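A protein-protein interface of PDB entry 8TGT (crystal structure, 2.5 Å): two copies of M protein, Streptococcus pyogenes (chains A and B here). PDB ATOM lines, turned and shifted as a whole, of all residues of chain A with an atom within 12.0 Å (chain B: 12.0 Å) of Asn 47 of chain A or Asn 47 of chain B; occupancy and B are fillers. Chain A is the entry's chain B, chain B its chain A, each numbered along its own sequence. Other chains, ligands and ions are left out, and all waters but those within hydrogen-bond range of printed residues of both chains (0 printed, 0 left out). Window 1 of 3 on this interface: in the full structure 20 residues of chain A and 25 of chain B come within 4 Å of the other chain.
OD1 of Asn 55 of chain B is in hydrogen-bond range of ND2 of Asn 58 of chain A (3.3 Å).
Among the printed residues, merely in contact across the chains: Asn 47 of chain A with Asn 47 of chain B, Asn 55 of chain A with Leu 54 of chain B and Asn 58 of chain A with Leu 54 of chain B.
Asn 47 of chain B touches just one residue of chain A: Asn 47.
No residue of chain B comes within 4 Å of Leu 45 of chain A.
No residue of chain B comes within 4 Å of Met 48 of chain A.
No residue of chain B comes within 4 Å of Glu 49 of chain A.
No residue of chain B comes within 4 Å of Asn 50 of chain A.
No residue of chain B comes within 4 Å of Leu 51 of chain A.
No residue of chain A comes within 4 Å of Met 43 of chain B.
No residue of chain A comes within 4 Å of Leu 45 of chain B.
No residue of chain A comes within 4 Å of Glu 46 of chain B.
No residue of chain A comes within 4 Å of Met 48 of chain B.
No residue of chain A comes within 4 Å of Asn 50 of chain B.
No residue of chain A comes within 4 Å of Leu 51 of chain B.
Of the printed residues of chain A, Asn 55 of chain B touches Asn 58.
Of the printed residues of chain B, Asn 55 of chain A touches Leu 54 (3.4 Å).
Glu 41 of chain B touches none of the printed residues of chain A.
The nearest residue of chain A that does not touch Asn 47 of chain B is Asn 50 of chain A (4.2 Å).
The nearest printed residue of chain B that does not touch Asn 58 of chain A is Leu 51 of chain B (6.3 Å).
Of the 18 printed residues of chain A, 3 touch a printed residue of chain B.
Of the 19 printed residues of chain B, 3 touch a printed residue of chain A.
Among the printed residues, 4 pairs touch across the chains.
Among the printed residues, no Asp or Glu carboxylate lies within 4 Å of a Lys or Arg side-chain nitrogen of the other chain.
Asn 47 of chain A touches its own counterpart, Asn 47 of chain B.
Asn 55 of chain A touches Leu 54 of chain B, but with the chains exchanged Leu 54 of chain A does not touch Asn 55 of chain B (5.9 Å).
Of the 4 pairs that touch across the chains among the printed residues, 1 has its exchanged pair printed and touching as well.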
ATOM      1  N   LYS A  38      27.661   9.359  13.380  1.00  0.00           N
ATOM      2  CA  LYS A  38      27.562  10.047  12.099  1.00  0.00           C
ATOM      3  C   LYS A  38      26.289   9.685  11.345  1.00  0.00           C
ATOM      4  O   LYS A  38      25.682  10.551  10.705  1.00  0.00           O
ATOM      5  CB  LYS A  38      28.786   9.731  11.236  1.00  0.00           C
ATOM      6  N   THR A  39      25.867   8.422  11.412  1.00  0.00           N
ATOM      7  CA  THR A  39      24.661   7.995  10.713  1.00  0.00           C
ATOM      8  C   THR A  39      23.384   8.507  11.367  1.00  0.00           C
ATOM      9  O   THR A  39      22.310   8.360  10.776  1.00  0.00           O
ATOM     10  CB  THR A  39      24.614   6.469  10.623  1.00  0.00           C
ATOM     11  OG1 THR A  39      24.771   5.908  11.931  1.00  0.00           O
ATOM     12  CG2 THR A  39      25.726   5.955   9.720  1.00  0.00           C
ATOM     13  N   VAL A  40      23.472   9.093  12.563  1.00  0.00           N
ATOM     14  CA  VAL A  40      22.291   9.685  13.187  1.00  0.00           C
ATOM     15  C   VAL A  40      21.831  10.903  12.395  1.00  0.00           C
ATOM     16  O   VAL A  40      20.638  11.069  12.113  1.00  0.00           O
ATOM     17  CB  VAL A  40      22.582  10.038  14.657  1.00  0.00           C
ATOM     18  CG1 VAL A  40      21.630  11.119  15.149  1.00  0.00           C
ATOM     19  CG2 VAL A  40      22.478   8.798  15.531  1.00  0.00           C
ATOM     20  N   GLU A  41      22.768  11.766  12.015  1.00  0.00           N
ATOM     21  CA  GLU A  41      22.445  12.946  11.220  1.00  0.00           C
ATOM     22  C   GLU A  41      23.249  12.973   9.923  1.00  0.00           C
ATOM     23  O   GLU A  41      23.214  12.023   9.138  1.00  0.00           O
ATOM     24  CB  GLU A  41      22.702  14.223  12.024  1.00  0.00           C
ATOM     25  N   SER A  44      19.142  11.989   9.361  1.00  0.00           N
ATOM     26  CA  SER A  44      18.355  13.206   9.517  1.00  0.00           C
ATOM     27  C   SER A  44      18.182  13.922   8.181  1.00  0.00           C
ATOM     28  O   SER A  44      17.061  14.160   7.734  1.00  0.00           O
ATOM     29  CB  SER A  44      19.007  14.141  10.537  1.00  0.00           C
ATOM     30  N   LEU A  45      19.306  14.272   7.550  1.00  0.00           N
ATOM     31  CA  LEU A  45      19.244  14.929   6.250  1.00  0.00           C
ATOM     32  C   LEU A  45      18.830  13.960   5.152  1.00  0.00           C
ATOM     33  O   LEU A  45      18.191  14.369   4.176  1.00  0.00           O
ATOM     34  CB  LEU A  45      20.594  15.566   5.916  1.00  0.00           C
ATOM     35  N   GLU A  46      19.181  12.679   5.290  1.00  0.00           N
ATOM     36  CA  GLU A  46      18.770  11.692   4.298  1.00  0.00           C
ATOM     37  C   GLU A  46      17.263  11.473   4.319  1.00  0.00           C
ATOM     38  O   GLU A  46      16.669  11.164   3.279  1.00  0.00           O
ATOM     39  CB  GLU A  46      19.505  10.372   4.532  1.00  0.00           C
ATOM     40  N   ASN A  47      16.630  11.630   5.483  1.00  0.00           N
ATOM     41  CA  ASN A  47      15.182  11.472   5.573  1.00  0.00           C
ATOM     42  C   ASN A  47      14.454  12.728   5.107  1.00  0.00           C
ATOM     43  O   ASN A  47      13.402  12.635   4.464  1.00  0.00           O
ATOM     44  CB  ASN A  47      14.779  11.124   7.006  1.00  0.00           C
ATOM     45  N   MET A  48      14.993  13.901   5.422  1.00  0.00           N
ATOM     46  CA  MET A  48      14.396  15.160   4.988  1.00  0.00           C
ATOM     47  C   MET A  48      14.487  15.300   3.474  1.00  0.00           C
ATOM     48  O   MET A  48      13.588  15.848   2.837  1.00  0.00           O
ATOM     49  CB  MET A  48      15.078  16.345   5.674  1.00  0.00           C
ATOM     50  N   GLU A  49      15.583  14.798   2.900  1.00  0.00           N
ATOM     51  CA  GLU A  49      15.741  14.821   1.450  1.00  0.00           C
ATOM     52  C   GLU A  49      14.930  13.725   0.771  1.00  0.00           C
ATOM     53  O   GLU A  49      14.520  13.889  -0.384  1.00  0.00           O
ATOM     54  CB  GLU A  49      17.218  14.688   1.076  1.00  0.00           C
ATOM     55  N   ASN A  50      14.691  12.608   1.464  1.00  0.00           N
ATOM     56  CA  ASN A  50      13.869  11.548   0.890  1.00  0.00           C
ATOM     57  C   ASN A  50      12.407  11.970   0.807  1.00  0.00           C
ATOM     58  O   ASN A  50      11.742  11.730  -0.207  1.00  0.00           O
ATOM     59  CB  ASN A  50      14.013  10.267   1.712  1.00  0.00           C
ATOM     60  N   LEU A  51      11.890  12.598   1.865  1.00  0.00           N
ATOM     61  CA  LEU A  51      10.513  13.079   1.837  1.00  0.00           C
ATOM     62  C   LEU A  51      10.346  14.238   0.863  1.00  0.00           C
ATOM     63  O   LEU A  51       9.283  14.382   0.248  1.00  0.00           O
ATOM     64  CB  LEU A  51      10.071  13.496   3.241  1.00  0.00           C
ATOM     65  N   ASP A  52      11.379  15.069   0.708  1.00  0.00           N
ATOM     66  CA  ASP A  52      11.304  16.172  -0.242  1.00  0.00           C
ATOM     67  C   ASP A  52      11.412  15.682  -1.679  1.00  0.00           C
ATOM     68  O   ASP A  52      10.791  16.260  -2.578  1.00  0.00           O
ATOM     69  CB  ASP A  52      12.400  17.198   0.055  1.00  0.00           C
ATOM     70  N   LYS A  53      12.190  14.622  -1.918  1.00  0.00           N
ATOM     71  CA  LYS A  53      12.311  14.091  -3.272  1.00  0.00           C
ATOM     72  C   LYS A  53      11.033  13.385  -3.706  1.00  0.00           C
ATOM     73  O   LYS A  53      10.638  13.468  -4.875  1.00  0.00           O
ATOM     74  CB  LYS A  53      13.507  13.143  -3.362  1.00  0.00           C
ATOM     75  N   LEU A  54      10.372  12.685  -2.780  1.00  0.00           N
ATOM     76  CA  LEU A  54       9.128  12.004  -3.125  1.00  0.00           C
ATOM     77  C   LEU A  54       7.993  12.991  -3.358  1.00  0.00           C
ATOM     78  O   LEU A  54       7.102  12.728  -4.173  1.00  0.00           O
ATOM     79  CB  LEU A  54       8.748  11.009  -2.028  1.00  0.00           C
ATOM     80  N   ASN A  55       8.004  14.126  -2.655  1.00  0.00           N
ATOM     81  CA  ASN A  55       6.961  15.127  -2.852  1.00  0.00           C
ATOM     82  C   ASN A  55       7.047  15.763  -4.233  1.00  0.00           C
ATOM     83  O   ASN A  55       6.018  16.141  -4.804  1.00  0.00           O
ATOM     84  CB  ASN A  55       7.051  16.200  -1.767  1.00  0.00           C
ATOM     85  CG  ASN A  55       6.122  15.929  -0.601  1.00  0.00           C
ATOM     86  OD1 ASN A  55       5.475  14.883  -0.538  1.00  0.00           O
ATOM     87  ND2 ASN A  55       6.053  16.872   0.332  1.00  0.00           N
ATOM     88  N   LYS A  56       8.256  15.888  -4.784  1.00  0.00           N
ATOM     89  CA  LYS A  56       8.403  16.470  -6.113  1.00  0.00           C
ATOM     90  C   LYS A  56       7.932  15.506  -7.193  1.00  0.00           C
ATOM     91  O   LYS A  56       7.242  15.910  -8.137  1.00  0.00           O
ATOM     92  CB  LYS A  56       9.856  16.878  -6.350  1.00  0.00           C
ATOM     93  N   ASN A  58       5.778  13.051  -6.801  1.00  0.00           N
ATOM     94  CA  ASN A  58       4.336  12.877  -6.673  1.00  0.00           C
ATOM     95  C   ASN A  58       3.580  14.068  -7.250  1.00  0.00           C
ATOM     96  O   ASN A  58       2.499  13.901  -7.827  1.00  0.00           O
ATOM     97  CB  ASN A  58       3.958  12.664  -5.207  1.00  0.00           C
ATOM     98  CG  ASN A  58       4.123  11.224  -4.768  1.00  0.00           C
ATOM     99  OD1 ASN A  58       4.656  10.396  -5.508  1.00  0.00           O
ATOM    100  ND2 ASN A  58       3.667  10.917  -3.560  1.00  0.00           N
ATOM    101  N   LYS B  38      18.722   2.453  18.838  1.00  0.00           N
ATOM    102  CA  LYS B  38      17.267   2.554  18.883  1.00  0.00           C
ATOM    103  C   LYS B  38      16.784   3.903  18.371  1.00  0.00           C
ATOM    104  O   LYS B  38      15.662   4.006  17.862  1.00  0.00           O
ATOM    105  CB  LYS B  38      16.766   2.313  20.307  1.00  0.00           C
ATOM    106  N   THR B  39      17.610   4.946  18.497  1.00  0.00           N
ATOM    107  CA  THR B  39      17.231   6.253  17.972  1.00  0.00           C
ATOM    108  C   THR B  39      17.195   6.245  16.449  1.00  0.00           C
ATOM    109  O   THR B  39      16.294   6.834  15.840  1.00  0.00           O
ATOM    110  CB  THR B  39      18.195   7.327  18.480  1.00  0.00           C
ATOM    111  N   VAL B  40      18.162   5.578  15.816  1.00  0.00           N
ATOM    112  CA  VAL B  40      18.166   5.489  14.360  1.00  0.00           C
ATOM    113  C   VAL B  40      17.131   4.483  13.870  1.00  0.00           C
ATOM    114  O   VAL B  40      16.581   4.641  12.775  1.00  0.00           O
ATOM    115  CB  VAL B  40      19.572   5.136  13.849  1.00  0.00           C
ATOM    116  N   GLU B  41      16.850   3.442  14.657  1.00  0.00           N
ATOM    117  CA  GLU B  41      15.846   2.462  14.254  1.00  0.00           C
ATOM    118  C   GLU B  41      14.447   3.065  14.271  1.00  0.00           C
ATOM    119  O   GLU B  41      13.647   2.816  13.361  1.00  0.00           O
ATOM    120  CB  GLU B  41      15.914   1.235  15.165  1.00  0.00           C
ATOM    121  N   ASN B  42      14.135   3.862  15.295  1.00  0.00           N
ATOM    122  CA  ASN B  42      12.831   4.514  15.350  1.00  0.00           C
ATOM    123  C   ASN B  42      12.715   5.625  14.316  1.00  0.00           C
ATOM    124  O   ASN B  42      11.625   5.860  13.781  1.00  0.00           O
ATOM    125  CB  ASN B  42      12.579   5.061  16.754  1.00  0.00           C
ATOM    126  CG  ASN B  42      12.338   3.964  17.772  1.00  0.00           C
ATOM    127  OD1 ASN B  42      12.064   2.819  17.413  1.00  0.00           O
ATOM    128  ND2 ASN B  42      12.443   4.309  19.050  1.00  0.00           N
ATOM    129  N   MET B  43      13.814   6.314  14.022  1.00  0.00           N
ATOM    130  CA  MET B  43      13.810   7.376  13.023  1.00  0.00           C
ATOM    131  C   MET B  43      13.650   6.799  11.620  1.00  0.00           C
ATOM    132  O   MET B  43      12.987   7.391  10.767  1.00  0.00           O
ATOM    133  CB  MET B  43      15.094   8.204  13.112  1.00  0.00           C
ATOM    134  N   SER B  44      14.266   5.637  11.386  1.00  0.00           N
ATOM    135  CA  SER B  44      14.133   4.982  10.089  1.00  0.00           C
ATOM    136  C   SER B  44      12.736   4.406   9.894  1.00  0.00           C
ATOM    137  O   SER B  44      12.227   4.387   8.768  1.00  0.00           O
ATOM    138  CB  SER B  44      15.184   3.883   9.943  1.00  0.00           C
ATOM    139  N   LEU B  45      12.105   3.934  10.972  1.00  0.00           N
ATOM    140  CA  LEU B  45      10.747   3.411  10.858  1.00  0.00           C
ATOM    141  C   LEU B  45       9.735   4.538  10.693  1.00  0.00           C
ATOM    142  O   LEU B  45       8.756   4.396   9.951  1.00  0.00           O
ATOM    143  CB  LEU B  45      10.410   2.556  12.079  1.00  0.00           C
ATOM    144  N   GLU B  46       9.953   5.664  11.378  1.00  0.00           N
ATOM    145  CA  GLU B  46       9.038   6.793  11.247  1.00  0.00           C
ATOM    146  C   GLU B  46       9.123   7.427   9.864  1.00  0.00           C
ATOM    147  O   GLU B  46       8.124   7.959   9.367  1.00  0.00           O
ATOM    148  CB  GLU B  46       9.329   7.835  12.328  1.00  0.00           C
ATOM    149  N   ASN B  47      10.297   7.381   9.232  1.00  0.00           N
ATOM    150  CA  ASN B  47      10.424   7.916   7.881  1.00  0.00           C
ATOM    151  C   ASN B  47       9.706   7.041   6.863  1.00  0.00           C
ATOM    152  O   ASN B  47       9.158   7.557   5.882  1.00  0.00           O
ATOM    153  CB  ASN B  47      11.899   8.060   7.506  1.00  0.00           C
ATOM    154  CG  ASN B  47      12.104   8.945   6.294  1.00  0.00           C
ATOM    155  OD1 ASN B  47      11.724  10.117   6.295  1.00  0.00           O
ATOM    156  ND2 ASN B  47      12.706   8.387   5.249  1.00  0.00           N
ATOM    157  N   MET B  48       9.699   5.728   7.074  1.00  0.00           N
ATOM    158  CA  MET B  48       8.986   4.813   6.192  1.00  0.00           C
ATOM    159  C   MET B  48       7.480   5.001   6.341  1.00  0.00           C
ATOM    160  O   MET B  48       6.735   4.921   5.365  1.00  0.00           O
ATOM    161  CB  MET B  48       9.376   3.364   6.488  1.00  0.00           C
ATOM    162  N   GLU B  49       7.042   5.254   7.577  1.00  0.00           N
ATOM    163  CA  GLU B  49       5.625   5.510   7.820  1.00  0.00           C
ATOM    164  C   GLU B  49       5.200   6.851   7.238  1.00  0.00           C
ATOM    165  O   GLU B  49       4.070   6.996   6.756  1.00  0.00           O
ATOM    166  CB  GLU B  49       5.331   5.457   9.319  1.00  0.00           C
ATOM    167  N   ASN B  50       6.089   7.847   7.278  1.00  0.00           N
ATOM    168  CA  ASN B  50       5.775   9.137   6.674  1.00  0.00           C
ATOM    169  C   ASN B  50       5.696   9.026   5.156  1.00  0.00           C
ATOM    170  O   ASN B  50       4.837   9.656   4.526  1.00  0.00           O
ATOM    171  CB  ASN B  50       6.815  10.176   7.087  1.00  0.00           C
ATOM    172  N   LEU B  51       6.578   8.227   4.551  1.00  0.00           N
ATOM    173  CA  LEU B  51       6.525   8.030   3.107  1.00  0.00           C
ATOM    174  C   LEU B  51       5.300   7.223   2.695  1.00  0.00           C
ATOM    175  O   LEU B  51       4.757   7.437   1.606  1.00  0.00           O
ATOM    176  CB  LEU B  51       7.801   7.341   2.622  1.00  0.00           C
ATOM    177  N   ASP B  52       4.853   6.296   3.547  1.00  0.00           N
ATOM    178  CA  ASP B  52       3.647   5.536   3.243  1.00  0.00           C
ATOM    179  C   ASP B  52       2.411   6.425   3.284  1.00  0.00           C
ATOM    180  O   ASP B  52       1.509   6.285   2.450  1.00  0.00           O
ATOM    181  CB  ASP B  52       3.503   4.366   4.216  1.00  0.00           C
ATOM    182  N   LYS B  53       2.352   7.348   4.250  1.00  0.00           N
ATOM    183  CA  LYS B  53       1.240   8.290   4.301  1.00  0.00           C
ATOM    184  C   LYS B  53       1.293   9.280   3.145  1.00  0.00           C
ATOM    185  O   LYS B  53       0.247   9.742   2.677  1.00  0.00           O
ATOM    186  CB  LYS B  53       1.240   9.034   5.637  1.00  0.00           C
ATOM    187  N   LEU B  54       2.496   9.616   2.673  1.00  0.00           N
ATOM    188  CA  LEU B  54       2.615  10.512   1.528  1.00  0.00           C
ATOM    189  C   LEU B  54       2.101   9.851   0.256  1.00  0.00           C
ATOM    190  O   LEU B  54       1.402  10.487  -0.541  1.00  0.00           O
ATOM    191  CB  LEU B  54       4.068  10.952   1.355  1.00  0.00           C
ATOM    192  CG  LEU B  54       4.450  12.334   1.891  1.00  0.00           C
ATOM    193  CD1 LEU B  54       3.897  12.555   3.293  1.00  0.00           C
ATOM    194  CD2 LEU B  54       5.960  12.513   1.872  1.00  0.00           C
ATOM    195  N   ASN B  55       2.437   8.576   0.050  1.00  0.00           N
ATOM    196  CA  ASN B  55       1.948   7.869  -1.128  1.00  0.00           C
ATOM    197  C   ASN B  55       0.467   7.536  -1.006  1.00  0.00           C
ATOM    198  O   ASN B  55      -0.248   7.525  -2.014  1.00  0.00           O
ATOM    199  CB  ASN B  55       2.765   6.599  -1.356  1.00  0.00           C
ATOM    200  CG  ASN B  55       3.546   6.635  -2.655  1.00  0.00           C
ATOM    201  OD1 ASN B  55       3.989   7.696  -3.097  1.00  0.00           O
ATOM    202  ND2 ASN B  55       3.715   5.474  -3.277  1.00  0.00           N
ATOM    203  N   LYS B  56      -0.009   7.263   0.211  1.00  0.00           N
ATOM    204  CA  LYS B  56      -1.434   7.015   0.404  1.00  0.00           C
ATOM    205  C   LYS B  56      -2.245   8.287   0.196  1.00  0.00           C
ATOM    206  O   LYS B  56      -3.313   8.255  -0.427  1.00  0.00           O
ATOM    207  CB  LYS B  56      -1.685   6.438   1.796  1.00  0.00           C
